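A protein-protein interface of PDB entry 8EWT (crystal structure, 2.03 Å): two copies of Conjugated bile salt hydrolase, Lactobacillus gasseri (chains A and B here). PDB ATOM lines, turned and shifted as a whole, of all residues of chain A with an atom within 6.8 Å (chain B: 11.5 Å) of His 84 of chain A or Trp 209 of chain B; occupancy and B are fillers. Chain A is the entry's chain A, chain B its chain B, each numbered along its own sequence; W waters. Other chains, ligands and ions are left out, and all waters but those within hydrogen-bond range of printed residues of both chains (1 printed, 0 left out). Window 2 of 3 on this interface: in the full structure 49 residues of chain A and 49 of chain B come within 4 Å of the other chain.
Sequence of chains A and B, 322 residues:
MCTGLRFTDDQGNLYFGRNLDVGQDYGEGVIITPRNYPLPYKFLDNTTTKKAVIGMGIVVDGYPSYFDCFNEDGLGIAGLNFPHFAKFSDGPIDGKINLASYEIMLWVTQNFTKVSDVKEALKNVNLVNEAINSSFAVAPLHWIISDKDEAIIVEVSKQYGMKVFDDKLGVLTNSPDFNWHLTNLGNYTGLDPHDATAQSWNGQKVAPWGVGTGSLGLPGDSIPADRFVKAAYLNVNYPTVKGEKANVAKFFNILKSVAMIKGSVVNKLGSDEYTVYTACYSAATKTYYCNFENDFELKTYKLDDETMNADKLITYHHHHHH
The backbone carbonyl oxygen (O) of Pro 83 of chain A lies within hydrogen-bond range of the side-chain hydroxyl (OG) of Ser 175 of chain A. NE2 of Gln 159 of chain A sits at hydrogen-bond distance from O of His 84 of chain A (3.1 Å). O of Phe 85 of chain A lies within hydrogen-bond range of N of Lys 158 of chain A (3.0 Å). The backbone NH (N) of Gly 212 of chain B sits at hydrogen-bond distance from the side-chain carboxylate (OD1) of Asp 195 of chain B, 2.8 Å away. N of Ala 196 of chain B is in hydrogen-bond range of OG1 of Thr 213 of chain B, 2.9 Å away.
Among the printed residues, pairs that only touch across the chains: Phe 85 of chain A with Trp 209 of chain B, Ile 223 of chain A with Gly 212 of chain B, Ile 223 of chain A with Val 211 of chain B, Ser 175 of chain A with Trp 209 of chain B, Ile 223 of chain A with Thr 213 of chain B, His 84 of chain A with Trp 209 of chain B, Pro 224 of chain A with Val 211 of chain B, Pro 83 of chain A with Trp 209 of chain B, Pro 224 of chain A with Gly 210 of chain B, Pro 176 of chain A with Trp 209 of chain B and His 84 of chain A with Pro 208 of chain B.
Printed residues of chain B within 4 Å of His 84 of chain A: Pro 208 and Trp 209. Trp 209 of chain B touches just these residues of chain A: Pro 83 (3.9 Å), His 84 (3.8 Å), Phe 85 (3.4 Å), Ser 175 (3.6 Å) and Pro 176 (3.9 Å). Of the printed residues of chain B, Phe 85 of chain A touches Trp 209. Ser 175 of chain A touches just one residue of chain B: Trp 209 (3.6 Å). Printed residues of chain B within 4 Å of Pro 176 of chain A: Trp 209. Printed residues of chain B within 4 Å of Pro 224 of chain A: Gly 210 and Val 211. Of the printed residues of chain A, Gly 210 of chain B touches Pro 224. Of the printed residues of chain A, Val 211 of chain B touches Ile 223 and Pro 224. Of the printed residues of chain A, Pro 208 of chain B touches His 84 (3.98 Å). Of the printed residues of chain A, Thr 213 of chain B touches Ile 223. The nearest printed residue of chain B that does not touch His 84 of chain A is Gly 210 of chain B (5.7 Å). The nearest residue of chain A that does not touch Trp 209 of chain B is Pro 224 of chain A (4.7 Å).
Hydrophobic or aromatic side chains of chain B that line the printed part of chain A: Trp 209. Hydrophobic or aromatic side chains of chain A within 4 Å of the printed part of chain B: Pro 83, His 84, Phe 85, Pro 176, Ile 223 and Pro 224. Among the printed residues, 11 pairs touch across the chains.
No position is printed for both chains.
Water W1 lies within hydrogen-bond range of O of Trp 209 of chain B (2.6 Å) and N of Ser 175 of chain A (3.1 Å).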
ATOM      1  N   PHE A  82      -0.014  21.555   5.102  1.00  0.00           N
ATOM      2  CA  PHE A  82       0.164  22.109   6.437  1.00  0.00           C
ATOM      3  C   PHE A  82       0.263  20.965   7.450  1.00  0.00           C
ATOM      4  O   PHE A  82      -0.481  20.954   8.442  1.00  0.00           O
ATOM      5  CB  PHE A  82      -1.015  23.040   6.737  1.00  0.00           C
ATOM      6  CG  PHE A  82      -0.861  23.912   7.954  1.00  0.00           C
ATOM      7  CD1 PHE A  82       0.384  24.326   8.412  1.00  0.00           C
ATOM      8  CD2 PHE A  82      -2.001  24.364   8.620  1.00  0.00           C
ATOM      9  CE1 PHE A  82       0.486  25.161   9.519  1.00  0.00           C
ATOM     10  CE2 PHE A  82      -1.909  25.190   9.723  1.00  0.00           C
ATOM     11  CZ  PHE A  82      -0.665  25.596  10.173  1.00  0.00           C
ATOM     12  N   PRO A  83       1.163  19.997   7.251  1.00  0.00           N
ATOM     13  CA  PRO A  83       1.165  18.806   8.111  1.00  0.00           C
ATOM     14  C   PRO A  83       1.594  19.125   9.533  1.00  0.00           C
ATOM     15  O   PRO A  83       2.290  20.110   9.806  1.00  0.00           O
ATOM     16  CB  PRO A  83       2.177  17.881   7.434  1.00  0.00           C
ATOM     17  CG  PRO A  83       3.150  18.822   6.810  1.00  0.00           C
ATOM     18  CD  PRO A  83       2.296  19.971   6.301  1.00  0.00           C
ATOM     19  N   HIS A  84       1.169  18.246  10.445  1.00  0.00           N
ATOM     20  CA  HIS A  84       1.383  18.304  11.889  1.00  0.00           C
ATOM     21  C   HIS A  84       0.655  19.475  12.522  1.00  0.00           C
ATOM     22  O   HIS A  84       0.827  19.714  13.721  1.00  0.00           O
ATOM     23  CB  HIS A  84       2.872  18.362  12.265  1.00  0.00           C
ATOM     24  CG  HIS A  84       3.728  17.411  11.481  1.00  0.00           C
ATOM     25  ND1 HIS A  84       3.688  16.044  11.665  1.00  0.00           N
ATOM     26  CD2 HIS A  84       4.632  17.629  10.495  1.00  0.00           C
ATOM     27  CE1 HIS A  84       4.533  15.463  10.831  1.00  0.00           C
ATOM     28  NE2 HIS A  84       5.119  16.402  10.110  1.00  0.00           N
ATOM     29  N   PHE A  85      -0.145  20.217  11.760  1.00  0.00           N
ATOM     30  CA  PHE A  85      -0.951  21.313  12.287  1.00  0.00           C
ATOM     31  C   PHE A  85      -2.418  21.187  11.888  1.00  0.00           C
ATOM     32  O   PHE A  85      -3.303  21.256  12.746  1.00  0.00           O
ATOM     33  CB  PHE A  85      -0.424  22.657  11.795  1.00  0.00           C
ATOM     34  CG  PHE A  85       0.735  23.181  12.577  1.00  0.00           C
ATOM     35  CD1 PHE A  85       2.018  22.714  12.329  1.00  0.00           C
ATOM     36  CD2 PHE A  85       0.545  24.139  13.562  1.00  0.00           C
ATOM     37  CE1 PHE A  85       3.099  23.207  13.041  1.00  0.00           C
ATOM     38  CE2 PHE A  85       1.628  24.631  14.299  1.00  0.00           C
ATOM     39  CZ  PHE A  85       2.904  24.167  14.029  1.00  0.00           C
ATOM     40  N   ALA A  86      -2.693  21.032  10.590  1.00  0.00           N
ATOM     41  CA  ALA A  86      -4.059  21.188  10.091  1.00  0.00           C
ATOM     42  C   ALA A  86      -4.997  20.179  10.736  1.00  0.00           C
ATOM     43  O   ALA A  86      -4.695  18.983  10.804  1.00  0.00           O
ATOM     44  CB  ALA A  86      -4.104  21.036   8.567  1.00  0.00           C
ATOM     45  N   PRO A 140      -4.288  17.691   4.668  1.00  0.00           N
ATOM     46  CA  PRO A 140      -4.033  18.687   5.748  1.00  0.00           C
ATOM     47  C   PRO A 140      -3.561  20.039   5.222  1.00  0.00           C
ATOM     48  O   PRO A 140      -2.393  20.434   5.343  1.00  0.00           O
ATOM     49  CB  PRO A 140      -2.964  17.989   6.596  1.00  0.00           C
ATOM     50  CG  PRO A 140      -2.246  17.072   5.650  1.00  0.00           C
ATOM     51  CD  PRO A 140      -3.214  16.691   4.548  1.00  0.00           C
ATOM     52  N   SER A 157      -5.920  24.869  12.737  1.00  0.00           N
ATOM     53  CA  SER A 157      -4.983  23.932  13.328  1.00  0.00           C
ATOM     54  C   SER A 157      -5.527  23.374  14.633  1.00  0.00           C
ATOM     55  O   SER A 157      -6.389  23.975  15.283  1.00  0.00           O
ATOM     56  CB  SER A 157      -3.616  24.598  13.581  1.00  0.00           C
ATOM     57  OG  SER A 157      -3.724  25.679  14.493  1.00  0.00           O
ATOM     58  N   LYS A 158      -4.999  22.204  15.007  1.00  0.00           N
ATOM     59  CA  LYS A 158      -5.248  21.672  16.345  1.00  0.00           C
ATOM     60  C   LYS A 158      -4.664  22.589  17.415  1.00  0.00           C
ATOM     61  O   LYS A 158      -5.253  22.757  18.486  1.00  0.00           O
ATOM     62  CB  LYS A 158      -4.665  20.264  16.475  1.00  0.00           C
ATOM     63  N   GLN A 159      -3.515  23.210  17.134  1.00  0.00           N
ATOM     64  CA  GLN A 159      -2.852  24.040  18.137  1.00  0.00           C
ATOM     65  C   GLN A 159      -3.606  25.340  18.392  1.00  0.00           C
ATOM     66  O   GLN A 159      -3.653  25.816  19.529  1.00  0.00           O
ATOM     67  CB  GLN A 159      -1.414  24.351  17.703  1.00  0.00           C
ATOM     68  CG  GLN A 159      -0.467  23.162  17.699  1.00  0.00           C
ATOM     69  CD  GLN A 159      -0.463  22.442  16.368  1.00  0.00           C
ATOM     70  OE1 GLN A 159      -1.402  22.573  15.570  1.00  0.00           O
ATOM     71  NE2 GLN A 159       0.596  21.677  16.111  1.00  0.00           N
ATOM     72  N   ASN A 174       4.936  25.920   3.673  1.00  0.00           N
ATOM     73  CA  ASN A 174       4.338  24.834   4.438  1.00  0.00           C
ATOM     74  C   ASN A 174       4.573  25.050   5.928  1.00  0.00           C
ATOM     75  O   ASN A 174       4.753  26.191   6.358  1.00  0.00           O
ATOM     76  CB  ASN A 174       4.908  23.487   3.964  1.00  0.00           C
ATOM     77  CG  ASN A 174       4.755  23.289   2.452  1.00  0.00           C
ATOM     78  OD1 ASN A 174       5.717  23.422   1.706  1.00  0.00           O
ATOM     79  ND2 ASN A 174       3.536  23.001   2.000  1.00  0.00           N
ATOM     80  N   SER A 175       4.584  23.975   6.719  1.00  0.00           N
ATOM     81  CA  SER A 175       4.621  24.100   8.166  1.00  0.00           C
ATOM     82  C   SER A 175       5.988  24.609   8.621  1.00  0.00           C
ATOM     83  O   SER A 175       6.995  24.404   7.942  1.00  0.00           O
ATOM     84  CB  SER A 175       4.308  22.756   8.823  1.00  0.00           C
ATOM     85  OG  SER A 175       3.046  22.253   8.385  1.00  0.00           O
ATOM     86  N   PRO A 176       6.060  25.245   9.796  1.00  0.00           N
ATOM     87  CA  PRO A 176       4.971  25.471  10.760  1.00  0.00           C
ATOM     88  C   PRO A 176       4.045  26.635  10.392  1.00  0.00           C
ATOM     89  O   PRO A 176       3.993  27.078   9.238  1.00  0.00           O
ATOM     90  CB  PRO A 176       5.725  25.713  12.085  1.00  0.00           C
ATOM     91  CG  PRO A 176       7.087  26.210  11.680  1.00  0.00           C
ATOM     92  CD  PRO A 176       7.389  25.570  10.354  1.00  0.00           C
ATOM     93  N   TRP A 180       4.627  31.815  12.857  1.00  0.00           N
ATOM     94  CA  TRP A 180       5.986  31.346  13.116  1.00  0.00           C
ATOM     95  C   TRP A 180       6.949  31.876  12.062  1.00  0.00           C
ATOM     96  O   TRP A 180       8.023  32.394  12.390  1.00  0.00           O
ATOM     97  CB  TRP A 180       6.048  29.813  13.167  1.00  0.00           C
ATOM     98  CG  TRP A 180       7.426  29.353  13.611  1.00  0.00           C
ATOM     99  CD1 TRP A 180       7.819  29.020  14.885  1.00  0.00           C
ATOM    100  CD2 TRP A 180       8.598  29.243  12.792  1.00  0.00           C
ATOM    101  NE1 TRP A 180       9.163  28.692  14.902  1.00  0.00           N
ATOM    102  CE2 TRP A 180       9.663  28.830  13.631  1.00  0.00           C
ATOM    103  CE3 TRP A 180       8.851  29.434  11.423  1.00  0.00           C
ATOM    104  CZ2 TRP A 180      10.943  28.595  13.147  1.00  0.00           C
ATOM    105  CZ3 TRP A 180      10.130  29.225  10.949  1.00  0.00           C
ATOM    106  CH2 TRP A 180      11.166  28.811  11.813  1.00  0.00           C
ATOM    107  N   ILE A 223      13.811  23.330   2.898  1.00  0.00           N
ATOM    108  CA  ILE A 223      13.080  23.375   4.171  1.00  0.00           C
ATOM    109  C   ILE A 223      12.037  24.491   4.088  1.00  0.00           C
ATOM    110  O   ILE A 223      12.356  25.602   3.625  1.00  0.00           O
ATOM    111  CB  ILE A 223      14.048  23.574   5.354  1.00  0.00           C
ATOM    112  CG1 ILE A 223      15.080  22.437   5.409  1.00  0.00           C
ATOM    113  CG2 ILE A 223      13.311  23.668   6.687  1.00  0.00           C
ATOM    114  CD1 ILE A 223      16.246  22.708   6.336  1.00  0.00           C
ATOM    115  N   PRO A 224      10.782  24.250   4.489  1.00  0.00           N
ATOM    116  CA  PRO A 224       9.738  25.277   4.264  1.00  0.00           C
ATOM    117  C   PRO A 224      10.072  26.636   4.872  1.00  0.00           C
ATOM    118  O   PRO A 224       9.783  27.674   4.256  1.00  0.00           O
ATOM    119  CB  PRO A 224       8.485  24.656   4.916  1.00  0.00           C
ATOM    120  CG  PRO A 224       8.742  23.187   4.959  1.00  0.00           C
ATOM    121  CD  PRO A 224      10.243  23.023   5.109  1.00  0.00           C
ATOM    122  N   ALA A 225      10.672  26.657   6.071  1.00  0.00           N
ATOM    123  CA  ALA A 225      11.095  27.924   6.675  1.00  0.00           C
ATOM    124  C   ALA A 225      12.065  28.686   5.769  1.00  0.00           C
ATOM    125  O   ALA A 225      11.989  29.914   5.650  1.00  0.00           O
ATOM    126  CB  ALA A 225      11.738  27.665   8.038  1.00  0.00           C
ATOM    127  N   ASP B 195      16.183  13.208   3.437  1.00  0.00           N
ATOM    128  CA  ASP B 195      15.615  13.933   4.563  1.00  0.00           C
ATOM    129  C   ASP B 195      16.123  13.359   5.879  1.00  0.00           C
ATOM    130  O   ASP B 195      16.466  12.179   5.977  1.00  0.00           O
ATOM    131  CB  ASP B 195      14.082  13.852   4.540  1.00  0.00           C
ATOM    132  CG  ASP B 195      13.454  14.760   3.493  1.00  0.00           C
ATOM    133  OD1 ASP B 195      14.113  15.704   3.019  1.00  0.00           O
ATOM    134  OD2 ASP B 195      12.278  14.525   3.141  1.00  0.00           O
ATOM    135  N   ALA B 196      16.177  14.210   6.897  1.00  0.00           N
ATOM    136  CA  ALA B 196      16.405  13.711   8.242  1.00  0.00           C
ATOM    137  C   ALA B 196      15.100  13.150   8.804  1.00  0.00           C
ATOM    138  O   ALA B 196      14.020  13.305   8.218  1.00  0.00           O
ATOM    139  CB  ALA B 196      16.960  14.817   9.135  1.00  0.00           C
ATOM    140  N   THR B 197      15.197  12.481   9.954  1.00  0.00           N
ATOM    141  CA  THR B 197      14.013  11.950  10.623  1.00  0.00           C
ATOM    142  C   THR B 197      13.988  12.396  12.084  1.00  0.00           C
ATOM    143  O   THR B 197      14.924  13.032  12.583  1.00  0.00           O
ATOM    144  CB  THR B 197      13.942  10.422  10.512  1.00  0.00           C
ATOM    145  OG1 THR B 197      15.231   9.854  10.784  1.00  0.00           O
ATOM    146  CG2 THR B 197      13.486  10.022   9.117  1.00  0.00           C
ATOM    147  N   ALA B 198      12.898  12.035  12.764  1.00  0.00           N
ATOM    148  CA  ALA B 198      12.622  12.527  14.109  1.00  0.00           C
ATOM    149  C   ALA B 198      13.737  12.142  15.065  1.00  0.00           C
ATOM    150  O   ALA B 198      14.364  11.088  14.927  1.00  0.00           O
ATOM    151  CB  ALA B 198      11.292  11.967  14.619  1.00  0.00           C
ATOM    152  N   GLN B 199      13.984  13.007  16.048  1.00  0.00           N
ATOM    153  CA  GLN B 199      15.083  12.803  16.984  1.00  0.00           C
ATOM    154  C   GLN B 199      14.602  13.067  18.403  1.00  0.00           C
ATOM    155  O   GLN B 199      13.567  13.700  18.630  1.00  0.00           O
ATOM    156  CB  GLN B 199      16.282  13.712  16.665  1.00  0.00           C
ATOM    157  CG  GLN B 199      16.937  13.419  15.338  1.00  0.00           C
ATOM    158  CD  GLN B 199      17.724  14.599  14.788  1.00  0.00           C
ATOM    159  OE1 GLN B 199      18.194  15.457  15.532  1.00  0.00           O
ATOM    160  NE2 GLN B 199      17.887  14.631  13.474  1.00  0.00           N
ATOM    161  N   TRP B 201      16.012  14.951  21.569  1.00  0.00           N
ATOM    162  CA  TRP B 201      17.004  15.830  22.197  1.00  0.00           C
ATOM    163  C   TRP B 201      16.720  15.823  23.693  1.00  0.00           C
ATOM    164  O   TRP B 201      15.922  16.616  24.199  1.00  0.00           O
ATOM    165  CB  TRP B 201      16.944  17.239  21.622  1.00  0.00           C
ATOM    166  CG  TRP B 201      17.387  17.367  20.179  1.00  0.00           C
ATOM    167  CD1 TRP B 201      17.202  16.458  19.171  1.00  0.00           C
ATOM    168  CD2 TRP B 201      18.077  18.485  19.591  1.00  0.00           C
ATOM    169  NE1 TRP B 201      17.736  16.942  17.996  1.00  0.00           N
ATOM    170  CE2 TRP B 201      18.276  18.183  18.227  1.00  0.00           C
ATOM    171  CE3 TRP B 201      18.539  19.711  20.085  1.00  0.00           C
ATOM    172  CZ2 TRP B 201      18.916  19.067  17.350  1.00  0.00           C
ATOM    173  CZ3 TRP B 201      19.173  20.588  19.206  1.00  0.00           C
ATOM    174  CH2 TRP B 201      19.356  20.256  17.861  1.00  0.00           C
ATOM    175  N   GLN B 204      13.130  15.448  24.291  1.00  0.00           N
ATOM    176  CA  GLN B 204      12.285  16.365  23.543  1.00  0.00           C
ATOM    177  C   GLN B 204      12.224  15.905  22.092  1.00  0.00           C
ATOM    178  O   GLN B 204      13.266  15.705  21.456  1.00  0.00           O
ATOM    179  CB  GLN B 204      12.840  17.788  23.619  1.00  0.00           C
ATOM    180  CG  GLN B 204      12.167  18.745  22.655  1.00  0.00           C
ATOM    181  CD  GLN B 204      10.748  19.097  23.080  1.00  0.00           C
ATOM    182  OE1 GLN B 204      10.517  19.517  24.211  1.00  0.00           O
ATOM    183  NE2 GLN B 204       9.800  18.957  22.166  1.00  0.00           N
ATOM    184  N   LYS B 205      11.010  15.722  21.571  1.00  0.00           N
ATOM    185  CA  LYS B 205      10.852  15.370  20.167  1.00  0.00           C
ATOM    186  C   LYS B 205      11.234  16.564  19.302  1.00  0.00           C
ATOM    187  O   LYS B 205      10.690  17.660  19.475  1.00  0.00           O
ATOM    188  CB  LYS B 205       9.419  14.927  19.876  1.00  0.00           C
ATOM    189  CG  LYS B 205       9.256  14.115  18.603  1.00  0.00           C
ATOM    190  CD  LYS B 205       7.915  14.423  17.927  1.00  0.00           C
ATOM    191  CE  LYS B 205       7.409  13.270  17.072  1.00  0.00           C
ATOM    192  NZ  LYS B 205       6.070  13.593  16.464  1.00  0.00           N
ATOM    193  N   VAL B 206      12.196  16.353  18.407  1.00  0.00           N
ATOM    194  CA  VAL B 206      12.637  17.331  17.419  1.00  0.00           C
ATOM    195  C   VAL B 206      12.523  16.636  16.069  1.00  0.00           C
ATOM    196  O   VAL B 206      13.242  15.662  15.810  1.00  0.00           O
ATOM    197  CB  VAL B 206      14.081  17.803  17.667  1.00  0.00           C
ATOM    198  CG1 VAL B 206      14.559  18.656  16.516  1.00  0.00           C
ATOM    199  CG2 VAL B 206      14.209  18.545  18.999  1.00  0.00           C
ATOM    200  N   ALA B 207      11.627  17.118  15.214  1.00  0.00           N
ATOM    201  CA  ALA B 207      11.293  16.413  13.983  1.00  0.00           C
ATOM    202  C   ALA B 207      11.126  17.396  12.836  1.00  0.00           C
ATOM    203  O   ALA B 207      10.706  18.543  13.049  1.00  0.00           O
ATOM    204  CB  ALA B 207      10.002  15.592  14.138  1.00  0.00           C
ATOM    205  N   PRO B 208      11.438  16.975  11.609  1.00  0.00           N
ATOM    206  CA  PRO B 208      11.284  17.871  10.455  1.00  0.00           C
ATOM    207  C   PRO B 208       9.840  18.331  10.297  1.00  0.00           C
ATOM    208  O   PRO B 208       8.902  17.570  10.534  1.00  0.00           O
ATOM    209  CB  PRO B 208      11.722  17.001   9.269  1.00  0.00           C
ATOM    210  CG  PRO B 208      12.516  15.880   9.867  1.00  0.00           C
ATOM    211  CD  PRO B 208      11.952  15.645  11.229  1.00  0.00           C
ATOM    212  N   TRP B 209       9.664  19.593   9.889  1.00  0.00           N
ATOM    213  CA  TRP B 209       8.333  20.112   9.577  1.00  0.00           C
ATOM    214  C   TRP B 209       7.924  19.878   8.128  1.00  0.00           C
ATOM    215  O   TRP B 209       6.725  19.948   7.808  1.00  0.00           O
ATOM    216  CB  TRP B 209       8.258  21.613   9.884  1.00  0.00           C
ATOM    217  CG  TRP B 209       8.373  21.901  11.342  1.00  0.00           C
ATOM    218  CD1 TRP B 209       9.421  22.497  11.978  1.00  0.00           C
ATOM    219  CD2 TRP B 209       7.412  21.577  12.361  1.00  0.00           C
ATOM    220  NE1 TRP B 209       9.168  22.573  13.337  1.00  0.00           N
ATOM    221  CE2 TRP B 209       7.941  22.020  13.593  1.00  0.00           C
ATOM    222  CE3 TRP B 209       6.159  20.961  12.349  1.00  0.00           C
ATOM    223  CZ2 TRP B 209       7.257  21.866  14.800  1.00  0.00           C
ATOM    224  CZ3 TRP B 209       5.479  20.807  13.549  1.00  0.00           C
ATOM    225  CH2 TRP B 209       6.031  21.261  14.759  1.00  0.00           C
ATOM    226  N   GLY B 210       8.890  19.612   7.256  1.00  0.00           N
ATOM    227  CA  GLY B 210       8.659  19.380   5.846  1.00  0.00           C
ATOM    228  C   GLY B 210       9.903  18.702   5.317  1.00  0.00           C
ATOM    229  O   GLY B 210      10.833  18.408   6.070  1.00  0.00           O
ATOM    230  N   VAL B 211       9.918  18.455   4.009  1.00  0.00           N
ATOM    231  CA  VAL B 211      11.081  17.829   3.393  1.00  0.00           C
ATOM    232  C   VAL B 211      12.168  18.881   3.169  1.00  0.00           C
ATOM    233  O   VAL B 211      11.924  20.089   3.224  1.00  0.00           O
ATOM    234  CB  VAL B 211      10.698  17.127   2.075  1.00  0.00           C
ATOM    235  CG1 VAL B 211       9.679  16.017   2.336  1.00  0.00           C
ATOM    236  CG2 VAL B 211      10.146  18.140   1.068  1.00  0.00           C
ATOM    237  N   GLY B 212      13.392  18.410   2.924  1.00  0.00           N
ATOM    238  CA  GLY B 212      14.506  19.284   2.608  1.00  0.00           C
ATOM    239  C   GLY B 212      15.580  19.367   3.666  1.00  0.00           C
ATOM    240  O   GLY B 212      16.629  19.973   3.404  1.00  0.00           O
ATOM    241  N   THR B 213      15.385  18.739   4.831  1.00  0.00           N
ATOM    242  CA  THR B 213      16.269  18.958   5.975  1.00  0.00           C
ATOM    243  C   THR B 213      17.673  18.398   5.761  1.00  0.00           C
ATOM    244  O   THR B 213      18.591  18.769   6.498  1.00  0.00           O
ATOM    245  CB  THR B 213      15.653  18.338   7.239  1.00  0.00           C
ATOM    246  OG1 THR B 213      15.268  16.987   6.968  1.00  0.00           O
ATOM    247  CG2 THR B 213      14.406  19.140   7.700  1.00  0.00           C
ATOM    248  N   GLY B 214      17.869  17.513   4.781  1.00  0.00           N
ATOM    249  CA  GLY B 214      19.207  16.990   4.563  1.00  0.00           C
ATOM    250  C   GLY B 214      20.188  18.002   3.999  1.00  0.00           C
ATOM    251  O   GLY B 214      21.408  17.829   4.150  1.00  0.00           O
HETATM  252  O   HOH W   1       5.522  21.144   5.813  1.00  0.00           O
